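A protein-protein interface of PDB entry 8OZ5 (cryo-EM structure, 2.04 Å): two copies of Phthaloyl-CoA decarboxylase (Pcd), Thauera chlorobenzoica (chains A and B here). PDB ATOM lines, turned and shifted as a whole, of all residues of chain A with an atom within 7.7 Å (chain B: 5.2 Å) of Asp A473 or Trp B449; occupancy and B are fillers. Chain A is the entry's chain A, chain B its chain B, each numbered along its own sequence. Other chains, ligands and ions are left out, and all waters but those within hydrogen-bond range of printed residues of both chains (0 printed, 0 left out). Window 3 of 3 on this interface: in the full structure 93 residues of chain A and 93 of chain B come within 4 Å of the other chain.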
ATOM      1  N   ARG A 417      11.466  15.546  -4.839  1.00  0.00           N
ATOM      2  CA  ARG A 417      10.805  16.672  -4.194  1.00  0.00           C
ATOM      3  C   ARG A 417      10.096  16.311  -2.895  1.00  0.00           C
ATOM      4  O   ARG A 417       9.262  17.093  -2.428  1.00  0.00           O
ATOM      5  CB  ARG A 417       9.804  17.320  -5.155  1.00  0.00           C
ATOM      6  CG  ARG A 417      10.459  18.041  -6.306  1.00  0.00           C
ATOM      7  CD  ARG A 417       9.444  18.592  -7.275  1.00  0.00           C
ATOM      8  NE  ARG A 417      10.082  19.422  -8.288  1.00  0.00           N
ATOM      9  CZ  ARG A 417       9.436  20.013  -9.284  1.00  0.00           C
ATOM     10  NH1 ARG A 417       8.126  19.868  -9.404  1.00  0.00           N
ATOM     11  NH2 ARG A 417      10.099  20.749 -10.161  1.00  0.00           N
ATOM     12  N   VAL A 466       7.011  22.052  -4.874  1.00  0.00           N
ATOM     13  CA  VAL A 466       8.187  22.894  -4.682  1.00  0.00           C
ATOM     14  C   VAL A 466       7.844  23.976  -3.667  1.00  0.00           C
ATOM     15  O   VAL A 466       6.788  24.614  -3.780  1.00  0.00           O
ATOM     16  CB  VAL A 466       8.653  23.508  -6.010  1.00  0.00           C
ATOM     17  CG1 VAL A 466       9.779  24.491  -5.769  1.00  0.00           C
ATOM     18  CG2 VAL A 466       9.088  22.420  -6.965  1.00  0.00           C
ATOM     19  N   GLY A 469       9.238  30.321  -3.432  1.00  0.00           N
ATOM     20  CA  GLY A 469      10.482  31.055  -3.358  1.00  0.00           C
ATOM     21  C   GLY A 469      11.710  30.256  -3.723  1.00  0.00           C
ATOM     22  O   GLY A 469      12.808  30.823  -3.759  1.00  0.00           O
ATOM     23  N   TYR A 470      11.563  28.961  -3.994  1.00  0.00           N
ATOM     24  CA  TYR A 470      12.669  28.112  -4.418  1.00  0.00           C
ATOM     25  C   TYR A 470      12.418  27.563  -5.814  1.00  0.00           C
ATOM     26  O   TYR A 470      12.932  26.503  -6.174  1.00  0.00           O
ATOM     27  CB  TYR A 470      12.895  26.973  -3.427  1.00  0.00           C
ATOM     28  CG  TYR A 470      13.289  27.438  -2.048  1.00  0.00           C
ATOM     29  CD1 TYR A 470      12.328  27.780  -1.110  1.00  0.00           C
ATOM     30  CD2 TYR A 470      14.623  27.540  -1.684  1.00  0.00           C
ATOM     31  CE1 TYR A 470      12.682  28.207   0.151  1.00  0.00           C
ATOM     32  CE2 TYR A 470      14.987  27.967  -0.425  1.00  0.00           C
ATOM     33  CZ  TYR A 470      14.014  28.299   0.488  1.00  0.00           C
ATOM     34  OH  TYR A 470      14.372  28.724   1.746  1.00  0.00           O
ATOM     35  N   GLU A 471      11.623  28.277  -6.610  1.00  0.00           N
ATOM     36  CA  GLU A 471      11.296  27.814  -7.952  1.00  0.00           C
ATOM     37  C   GLU A 471      12.494  27.863  -8.887  1.00  0.00           C
ATOM     38  O   GLU A 471      12.499  27.162  -9.903  1.00  0.00           O
ATOM     39  CB  GLU A 471      10.150  28.644  -8.529  1.00  0.00           C
ATOM     40  CG  GLU A 471       8.857  28.573  -7.727  1.00  0.00           C
ATOM     41  CD  GLU A 471       8.810  29.576  -6.589  1.00  0.00           C
ATOM     42  OE1 GLU A 471       9.794  30.323  -6.410  1.00  0.00           O
ATOM     43  OE2 GLU A 471       7.789  29.615  -5.873  1.00  0.00           O
ATOM     44  N   SER A 472      13.504  28.672  -8.571  1.00  0.00           N
ATOM     45  CA  SER A 472      14.702  28.716  -9.399  1.00  0.00           C
ATOM     46  C   SER A 472      15.614  27.531  -9.117  1.00  0.00           C
ATOM     47  O   SER A 472      16.294  27.038 -10.022  1.00  0.00           O
ATOM     48  CB  SER A 472      15.450  30.029  -9.170  1.00  0.00           C
ATOM     49  OG  SER A 472      15.895  30.130  -7.830  1.00  0.00           O
ATOM     50  N   ASP A 473      15.641  27.061  -7.870  1.00  0.00           N
ATOM     51  CA  ASP A 473      16.477  25.920  -7.525  1.00  0.00           C
ATOM     52  C   ASP A 473      15.845  24.601  -7.943  1.00  0.00           C
ATOM     53  O   ASP A 473      16.562  23.630  -8.203  1.00  0.00           O
ATOM     54  CB  ASP A 473      16.762  25.918  -6.025  1.00  0.00           C
ATOM     55  CG  ASP A 473      17.387  27.213  -5.555  1.00  0.00           C
ATOM     56  OD1 ASP A 473      16.649  28.207  -5.404  1.00  0.00           O
ATOM     57  OD2 ASP A 473      18.617  27.242  -5.352  1.00  0.00           O
ATOM     58  N   PHE A 474      14.515  24.544  -8.013  1.00  0.00           N
ATOM     59  CA  PHE A 474      13.799  23.352  -8.445  1.00  0.00           C
ATOM     60  C   PHE A 474      13.342  23.454  -9.893  1.00  0.00           C
ATOM     61  O   PHE A 474      12.300  22.903 -10.254  1.00  0.00           O
ATOM     62  CB  PHE A 474      12.603  23.093  -7.530  1.00  0.00           C
ATOM     63  CG  PHE A 474      12.977  22.536  -6.192  1.00  0.00           C
ATOM     64  CD1 PHE A 474      13.293  23.378  -5.143  1.00  0.00           C
ATOM     65  CD2 PHE A 474      13.014  21.172  -5.983  1.00  0.00           C
ATOM     66  CE1 PHE A 474      13.638  22.869  -3.913  1.00  0.00           C
ATOM     67  CE2 PHE A 474      13.358  20.657  -4.754  1.00  0.00           C
ATOM     68  CZ  PHE A 474      13.669  21.507  -3.718  1.00  0.00           C
ATOM     69  N   HIS A 475      14.103  24.154 -10.726  1.00  0.00           N
ATOM     70  CA  HIS A 475      13.691  24.413 -12.097  1.00  0.00           C
ATOM     71  C   HIS A 475      14.148  23.292 -13.025  1.00  0.00           C
ATOM     72  O   HIS A 475      15.346  23.026 -13.150  1.00  0.00           O
ATOM     73  CB  HIS A 475      14.260  25.757 -12.548  1.00  0.00           C
ATOM     74  CG  HIS A 475      13.791  26.199 -13.896  1.00  0.00           C
ATOM     75  ND1 HIS A 475      12.532  26.714 -14.116  1.00  0.00           N
ATOM     76  CD2 HIS A 475      14.424  26.232 -15.092  1.00  0.00           C
ATOM     77  CE1 HIS A 475      12.402  27.025 -15.393  1.00  0.00           C
ATOM     78  NE2 HIS A 475      13.536  26.741 -16.007  1.00  0.00           N
ATOM     79  N   ARG A 476      13.187  22.626 -13.670  1.00  0.00           N
ATOM     80  CA  ARG A 476      13.444  21.691 -14.760  1.00  0.00           C
ATOM     81  C   ARG A 476      13.682  22.480 -16.040  1.00  0.00           C
ATOM     82  O   ARG A 476      12.725  22.956 -16.654  1.00  0.00           O
ATOM     83  CB  ARG A 476      12.259  20.757 -14.963  1.00  0.00           C
ATOM     84  CG  ARG A 476      11.660  20.215 -13.683  1.00  0.00           C
ATOM     85  CD  ARG A 476      10.412  19.408 -13.979  1.00  0.00           C
ATOM     86  NE  ARG A 476      10.722  18.111 -14.567  1.00  0.00           N
ATOM     87  CZ  ARG A 476       9.806  17.241 -14.976  1.00  0.00           C
ATOM     88  NH1 ARG A 476       8.519  17.531 -14.869  1.00  0.00           N
ATOM     89  NH2 ARG A 476      10.178  16.083 -15.499  1.00  0.00           N
ATOM     90  N   GLN B 276      28.987  29.534  -4.832  1.00  0.00           N
ATOM     91  CA  GLN B 276      28.702  28.252  -5.453  1.00  0.00           C
ATOM     92  C   GLN B 276      27.246  27.863  -5.231  1.00  0.00           C
ATOM     93  O   GLN B 276      26.543  28.430  -4.393  1.00  0.00           O
ATOM     94  CB  GLN B 276      29.626  27.168  -4.899  1.00  0.00           C
ATOM     95  CG  GLN B 276      31.045  27.635  -4.647  1.00  0.00           C
ATOM     96  CD  GLN B 276      31.968  26.499  -4.263  1.00  0.00           C
ATOM     97  OE1 GLN B 276      31.817  25.375  -4.738  1.00  0.00           O
ATOM     98  NE2 GLN B 276      32.932  26.786  -3.399  1.00  0.00           N
ATOM     99  N   GLY B 277      26.797  26.875  -6.001  1.00  0.00           N
ATOM    100  CA  GLY B 277      25.438  26.389  -5.886  1.00  0.00           C
ATOM    101  C   GLY B 277      24.398  27.196  -6.625  1.00  0.00           C
ATOM    102  O   GLY B 277      23.231  26.794  -6.652  1.00  0.00           O
ATOM    103  N   ARG B 278      24.776  28.333  -7.205  1.00  0.00           N
ATOM    104  CA  ARG B 278      23.875  29.130  -8.024  1.00  0.00           C
ATOM    105  C   ARG B 278      24.527  29.318  -9.385  1.00  0.00           C
ATOM    106  O   ARG B 278      25.549  28.697  -9.687  1.00  0.00           O
ATOM    107  CB  ARG B 278      23.562  30.480  -7.366  1.00  0.00           C
ATOM    108  CG  ARG B 278      22.423  30.431  -6.350  1.00  0.00           C
ATOM    109  CD  ARG B 278      22.797  29.604  -5.129  1.00  0.00           C
ATOM    110  NE  ARG B 278      21.726  29.554  -4.136  1.00  0.00           N
ATOM    111  CZ  ARG B 278      21.669  30.332  -3.059  1.00  0.00           C
ATOM    112  NH1 ARG B 278      22.625  31.220  -2.827  1.00  0.00           N
ATOM    113  NH2 ARG B 278      20.657  30.216  -2.211  1.00  0.00           N
ATOM    114  N   TYR B 288      17.154  18.559 -12.940  1.00  0.00           N
ATOM    115  CA  TYR B 288      16.990  19.980 -12.688  1.00  0.00           C
ATOM    116  C   TYR B 288      18.057  20.773 -13.428  1.00  0.00           C
ATOM    117  O   TYR B 288      19.095  20.233 -13.818  1.00  0.00           O
ATOM    118  CB  TYR B 288      17.077  20.288 -11.194  1.00  0.00           C
ATOM    119  CG  TYR B 288      15.937  19.727 -10.388  1.00  0.00           C
ATOM    120  CD1 TYR B 288      14.725  20.394 -10.308  1.00  0.00           C
ATOM    121  CD2 TYR B 288      16.068  18.527  -9.711  1.00  0.00           C
ATOM    122  CE1 TYR B 288      13.680  19.885  -9.574  1.00  0.00           C
ATOM    123  CE2 TYR B 288      15.030  18.010  -8.973  1.00  0.00           C
ATOM    124  CZ  TYR B 288      13.838  18.692  -8.908  1.00  0.00           C
ATOM    125  OH  TYR B 288      12.800  18.175  -8.174  1.00  0.00           O
ATOM    126  N   MET B 289      17.790  22.062 -13.617  1.00  0.00           N
ATOM    127  CA  MET B 289      18.806  22.952 -14.159  1.00  0.00           C
ATOM    128  C   MET B 289      19.975  23.046 -13.191  1.00  0.00           C
ATOM    129  O   MET B 289      19.795  23.015 -11.971  1.00  0.00           O
ATOM    130  CB  MET B 289      18.233  24.338 -14.437  1.00  0.00           C
ATOM    131  CG  MET B 289      19.258  25.289 -15.038  1.00  0.00           C
ATOM    132  SD  MET B 289      19.827  24.741 -16.659  1.00  0.00           S
ATOM    133  CE  MET B 289      21.522  25.304 -16.652  1.00  0.00           C
ATOM    134  N   LYS B 291      23.975  24.065 -11.541  1.00  0.00           N
ATOM    135  CA  LYS B 291      24.657  25.123 -10.818  1.00  0.00           C
ATOM    136  C   LYS B 291      26.161  24.968 -11.010  1.00  0.00           C
ATOM    137  O   LYS B 291      26.653  23.912 -11.415  1.00  0.00           O
ATOM    138  CB  LYS B 291      24.294  25.090  -9.329  1.00  0.00           C
ATOM    139  CG  LYS B 291      22.801  25.139  -9.068  1.00  0.00           C
ATOM    140  CD  LYS B 291      22.208  26.452  -9.538  1.00  0.00           C
ATOM    141  CE  LYS B 291      20.705  26.476  -9.353  1.00  0.00           C
ATOM    142  NZ  LYS B 291      20.021  25.555 -10.299  1.00  0.00           N
ATOM    143  N   TYR B 293      30.171  25.410  -9.440  1.00  0.00           N
ATOM    144  CA  TYR B 293      30.940  25.292  -8.210  1.00  0.00           C
ATOM    145  C   TYR B 293      32.414  25.516  -8.515  1.00  0.00           C
ATOM    146  O   TYR B 293      32.826  25.618  -9.673  1.00  0.00           O
ATOM    147  CB  TYR B 293      30.744  23.917  -7.560  1.00  0.00           C
ATOM    148  CG  TYR B 293      29.311  23.555  -7.254  1.00  0.00           C
ATOM    149  CD1 TYR B 293      28.489  23.014  -8.230  1.00  0.00           C
ATOM    150  CD2 TYR B 293      28.785  23.741  -5.986  1.00  0.00           C
ATOM    151  CE1 TYR B 293      27.183  22.679  -7.955  1.00  0.00           C
ATOM    152  CE2 TYR B 293      27.479  23.407  -5.702  1.00  0.00           C
ATOM    153  CZ  TYR B 293      26.682  22.877  -6.689  1.00  0.00           C
ATOM    154  OH  TYR B 293      25.378  22.541  -6.415  1.00  0.00           O
ATOM    155  N   THR B 435      24.777  16.496  -3.365  1.00  0.00           N
ATOM    156  CA  THR B 435      24.585  17.943  -3.358  1.00  0.00           C
ATOM    157  C   THR B 435      23.723  18.407  -4.521  1.00  0.00           C
ATOM    158  O   THR B 435      23.085  19.464  -4.439  1.00  0.00           O
ATOM    159  CB  THR B 435      25.937  18.651  -3.389  1.00  0.00           C
ATOM    160  OG1 THR B 435      26.794  18.086  -2.390  1.00  0.00           O
ATOM    161  CG2 THR B 435      25.761  20.133  -3.111  1.00  0.00           C
ATOM    162  N   PRO B 438      18.149  19.232  -5.360  1.00  0.00           N
ATOM    163  CA  PRO B 438      17.722  20.516  -4.783  1.00  0.00           C
ATOM    164  C   PRO B 438      17.044  20.377  -3.436  1.00  0.00           C
ATOM    165  O   PRO B 438      17.197  21.260  -2.584  1.00  0.00           O
ATOM    166  CB  PRO B 438      16.760  21.076  -5.841  1.00  0.00           C
ATOM    167  CG  PRO B 438      17.076  20.327  -7.089  1.00  0.00           C
ATOM    168  CD  PRO B 438      17.509  18.967  -6.656  1.00  0.00           C
ATOM    169  N   ARG B 441      20.046  20.093  -1.228  1.00  0.00           N
ATOM    170  CA  ARG B 441      20.861  21.300  -1.262  1.00  0.00           C
ATOM    171  C   ARG B 441      20.176  22.484  -0.594  1.00  0.00           C
ATOM    172  O   ARG B 441      20.863  23.383  -0.098  1.00  0.00           O
ATOM    173  CB  ARG B 441      21.214  21.648  -2.708  1.00  0.00           C
ATOM    174  CG  ARG B 441      22.359  22.628  -2.851  1.00  0.00           C
ATOM    175  CD  ARG B 441      22.295  23.328  -4.191  1.00  0.00           C
ATOM    176  NE  ARG B 441      21.708  22.470  -5.215  1.00  0.00           N
ATOM    177  CZ  ARG B 441      20.844  22.889  -6.132  1.00  0.00           C
ATOM    178  NH1 ARG B 441      20.462  24.158  -6.154  1.00  0.00           N
ATOM    179  NH2 ARG B 441      20.360  22.041  -7.027  1.00  0.00           N
ATOM    180  N   MET B 442      18.846  22.508  -0.567  1.00  0.00           N
ATOM    181  CA  MET B 442      18.121  23.576   0.106  1.00  0.00           C
ATOM    182  C   MET B 442      18.209  23.484   1.622  1.00  0.00           C
ATOM    183  O   MET B 442      17.821  24.436   2.306  1.00  0.00           O
ATOM    184  CB  MET B 442      16.654  23.572  -0.331  1.00  0.00           C
ATOM    185  CG  MET B 442      15.807  22.496   0.321  1.00  0.00           C
ATOM    186  SD  MET B 442      14.061  22.693  -0.071  1.00  0.00           S
ATOM    187  CE  MET B 442      13.818  24.408   0.375  1.00  0.00           C
ATOM    188  N   SER B 444      20.926  23.592   3.148  1.00  0.00           N
ATOM    189  CA  SER B 444      22.054  24.429   3.534  1.00  0.00           C
ATOM    190  C   SER B 444      21.607  25.681   4.273  1.00  0.00           C
ATOM    191  O   SER B 444      22.384  26.246   5.049  1.00  0.00           O
ATOM    192  CB  SER B 444      22.864  24.816   2.300  1.00  0.00           C
ATOM    193  OG  SER B 444      23.416  23.672   1.678  1.00  0.00           O
ATOM    194  N   GLY B 445      20.373  26.123   4.054  1.00  0.00           N
ATOM    195  CA  GLY B 445      19.864  27.300   4.729  1.00  0.00           C
ATOM    196  C   GLY B 445      20.470  28.585   4.209  1.00  0.00           C
ATOM    197  O   GLY B 445      20.261  28.953   3.049  1.00  0.00           O
ATOM    198  N   ASP B 446      21.225  29.279   5.057  1.00  0.00           N
ATOM    199  CA  ASP B 446      21.881  30.522   4.684  1.00  0.00           C
ATOM    200  C   ASP B 446      23.378  30.353   4.462  1.00  0.00           C
ATOM    201  O   ASP B 446      24.089  31.350   4.302  1.00  0.00           O
ATOM    202  CB  ASP B 446      21.620  31.591   5.748  1.00  0.00           C
ATOM    203  CG  ASP B 446      20.141  31.872   5.939  1.00  0.00           C
ATOM    204  OD1 ASP B 446      19.583  31.469   6.982  1.00  0.00           O
ATOM    205  OD2 ASP B 446      19.534  32.500   5.047  1.00  0.00           O
ATOM    206  N   LYS B 447      23.870  29.118   4.440  1.00  0.00           N
ATOM    207  CA  LYS B 447      25.269  28.831   4.178  1.00  0.00           C
ATOM    208  C   LYS B 447      25.483  28.651   2.677  1.00  0.00           C
ATOM    209  O   LYS B 447      24.555  28.758   1.872  1.00  0.00           O
ATOM    210  CB  LYS B 447      25.713  27.584   4.945  1.00  0.00           C
ATOM    211  CG  LYS B 447      25.709  27.737   6.452  1.00  0.00           C
ATOM    212  CD  LYS B 447      26.191  26.470   7.130  1.00  0.00           C
ATOM    213  CE  LYS B 447      25.769  26.434   8.586  1.00  0.00           C
ATOM    214  NZ  LYS B 447      26.806  25.806   9.444  1.00  0.00           N
ATOM    215  N   GLN B 448      26.730  28.388   2.296  1.00  0.00           N
ATOM    216  CA  GLN B 448      27.023  28.035   0.915  1.00  0.00           C
ATOM    217  C   GLN B 448      26.345  26.719   0.563  1.00  0.00           C
ATOM    218  O   GLN B 448      26.406  25.748   1.321  1.00  0.00           O
ATOM    219  CB  GLN B 448      28.532  27.925   0.697  1.00  0.00           C
ATOM    220  CG  GLN B 448      29.229  29.258   0.496  1.00  0.00           C
ATOM    221  CD  GLN B 448      29.264  29.682  -0.958  1.00  0.00           C
ATOM    222  OE1 GLN B 448      28.224  29.918  -1.572  1.00  0.00           O
ATOM    223  NE2 GLN B 448      30.464  29.783  -1.516  1.00  0.00           N
ATOM    224  N   TRP B 449      25.691  26.687  -0.599  1.00  0.00           N
ATOM    225  CA  TRP B 449      24.938  25.508  -1.025  1.00  0.00           C
ATOM    226  C   TRP B 449      25.888  24.520  -1.704  1.00  0.00           C
ATOM    227  O   TRP B 449      25.850  24.283  -2.912  1.00  0.00           O
ATOM    228  CB  TRP B 449      23.788  25.905  -1.940  1.00  0.00           C
ATOM    229  CG  TRP B 449      22.615  26.504  -1.218  1.00  0.00           C
ATOM    230  CD1 TRP B 449      22.644  27.234  -0.066  1.00  0.00           C
ATOM    231  CD2 TRP B 449      21.236  26.415  -1.598  1.00  0.00           C
ATOM    232  NE1 TRP B 449      21.373  27.608   0.292  1.00  0.00           N
ATOM    233  CE2 TRP B 449      20.490  27.116  -0.632  1.00  0.00           C
ATOM    234  CE3 TRP B 449      20.561  25.809  -2.662  1.00  0.00           C
ATOM    235  CZ2 TRP B 449      19.104  27.232  -0.699  1.00  0.00           C
ATOM    236  CZ3 TRP B 449      19.185  25.923  -2.723  1.00  0.00           C
ATOM    237  CH2 TRP B 449      18.472  26.629  -1.750  1.00  0.00           C
ATOM    238  N   THR B 450      26.761  23.939  -0.889  1.00  0.00           N
ATOM    239  CA  THR B 450      27.735  22.952  -1.333  1.00  0.00           C
ATOM    240  C   THR B 450      27.563  21.670  -0.519  1.00  0.00           C
ATOM    241  O   THR B 450      26.658  21.553   0.311  1.00  0.00           O
ATOM    242  CB  THR B 450      29.157  23.506  -1.211  1.00  0.00           C
ATOM    243  OG1 THR B 450      29.492  23.665   0.172  1.00  0.00           O
ATOM    244  CG2 THR B 450      29.261  24.849  -1.906  1.00  0.00           C
ATOM    245  N   ALA B 451      28.446  20.701  -0.762  1.00  0.00           N
ATOM    246  CA  ALA B 451      28.387  19.438  -0.039  1.00  0.00           C
ATOM    247  C   ALA B 451      28.803  19.570   1.418  1.00  0.00           C
ATOM    248  O   ALA B 451      28.568  18.640   2.196  1.00  0.00           O
ATOM    249  CB  ALA B 451      29.267  18.392  -0.725  1.00  0.00           C
ATOM    250  N   ASN B 453      27.566  21.772   3.520  1.00  0.00           N
ATOM    251  CA  ASN B 453      26.478  22.332   4.304  1.00  0.00           C
ATOM    252  C   ASN B 453      25.153  21.605   4.143  1.00  0.00           C
ATOM    253  O   ASN B 453      24.245  21.837   4.949  1.00  0.00           O
ATOM    254  CB  ASN B 453      26.278  23.813   3.951  1.00  0.00           C
ATOM    255  CG  ASN B 453      27.552  24.614   4.081  1.00  0.00           C
ATOM    256  OD1 ASN B 453      28.238  24.547   5.099  1.00  0.00           O
ATOM    257  ND2 ASN B 453      27.879  25.376   3.046  1.00  0.00           N
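Tyr A470 touches Met B442. Trp B449 touches Tyr A470 (CH2 to CD2, 3.96 Å). Asp A473 touches Pro B438. Trp B449 touches Asp A473. C of Phe A474 touches CD1 of Tyr B288, at 3.4 Å. Phe A474 touches Pro B438. CZ of Phe A474 touches SD of Met B442, 3.9 Å away. His A475 touches Tyr B288 (O to CA, 3.5 Å).
OH of Tyr B288 is in hydrogen-bond range of NE of Arg A417 (3.0 Å). OD2 of Asp A473 lies within salt-bridge range of NH1 of Arg B441 (3.7 Å). N of Met B289 lies within hydrogen-bond range of O of His A475, at 2.7 Å.
No position is printed for both chains. Of the 11 pairs that touch across the chains among the printed residues, none has its exchanged pair printed and touching as well.
Printed residues of chain B within 4 Å of Arg A417: Tyr B288 (3.0 Å). Gly A469 touches none of the printed residues of chain B. Of the printed residues of chain B, Tyr A470 touches Met B442 (3.8 Å) and Trp B449 (3.96 Å). Of chain B, only Pro B438 (3.5 Å), Arg B441 (3.7 Å) and Trp B449 (3.0 Å) come within 4 Å of Asp A473. Of the printed residues of chain A, Met B289 touches His A475 (2.7 Å). Thr B435 touches none of the printed residues of chain A. Of chain A, only Tyr A470 and Asp A473 come within 4 Å of Trp B449. The nearest residue of chain A that does not touch Trp B449 is Phe A474 (6.4 Å).
Hydrophobic or aromatic side chains of chain A that line the printed part of chain B: Tyr A470 and Phe A474. Along chain A the printed residues that touch a printed residue of chain B span positions 417 to 475. Hydrophobic or aromatic side chains of chain B within 4 Å of the printed part of chain A: Tyr B288, Met B289, Pro B438, Met B442 and Trp B449. Among the printed residues, Asp or Glu carboxylates within 4 Å of a Lys or Arg side-chain nitrogen of the other chain: Asp A473 with Arg B441 (3.7 Å).
NH2 of Arg A417 lies within hydrogen-bond range of O of Phe A474 (3.1 Å). OG of Ser A472 sits at hydrogen-bond distance from OD1 of Asp A473 (3.2 Å). O of Met B289 lies within hydrogen-bond range of NZ of Lys B291 (3.0 Å). The backbone carbonyl oxygen of Thr B435 sits close to the guanidinium group of Arg B441, 3.4 Å away. The side-chain hydroxyl (OG) of Ser B444 sits at hydrogen-bond distance from the backbone carbonyl oxygen (O) of Arg B441. The backbone carbonyl oxygen (O) of Gly B445 lies within hydrogen-bond range of the indole nitrogen (NE1) of Trp B449, 3.3 Å away.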
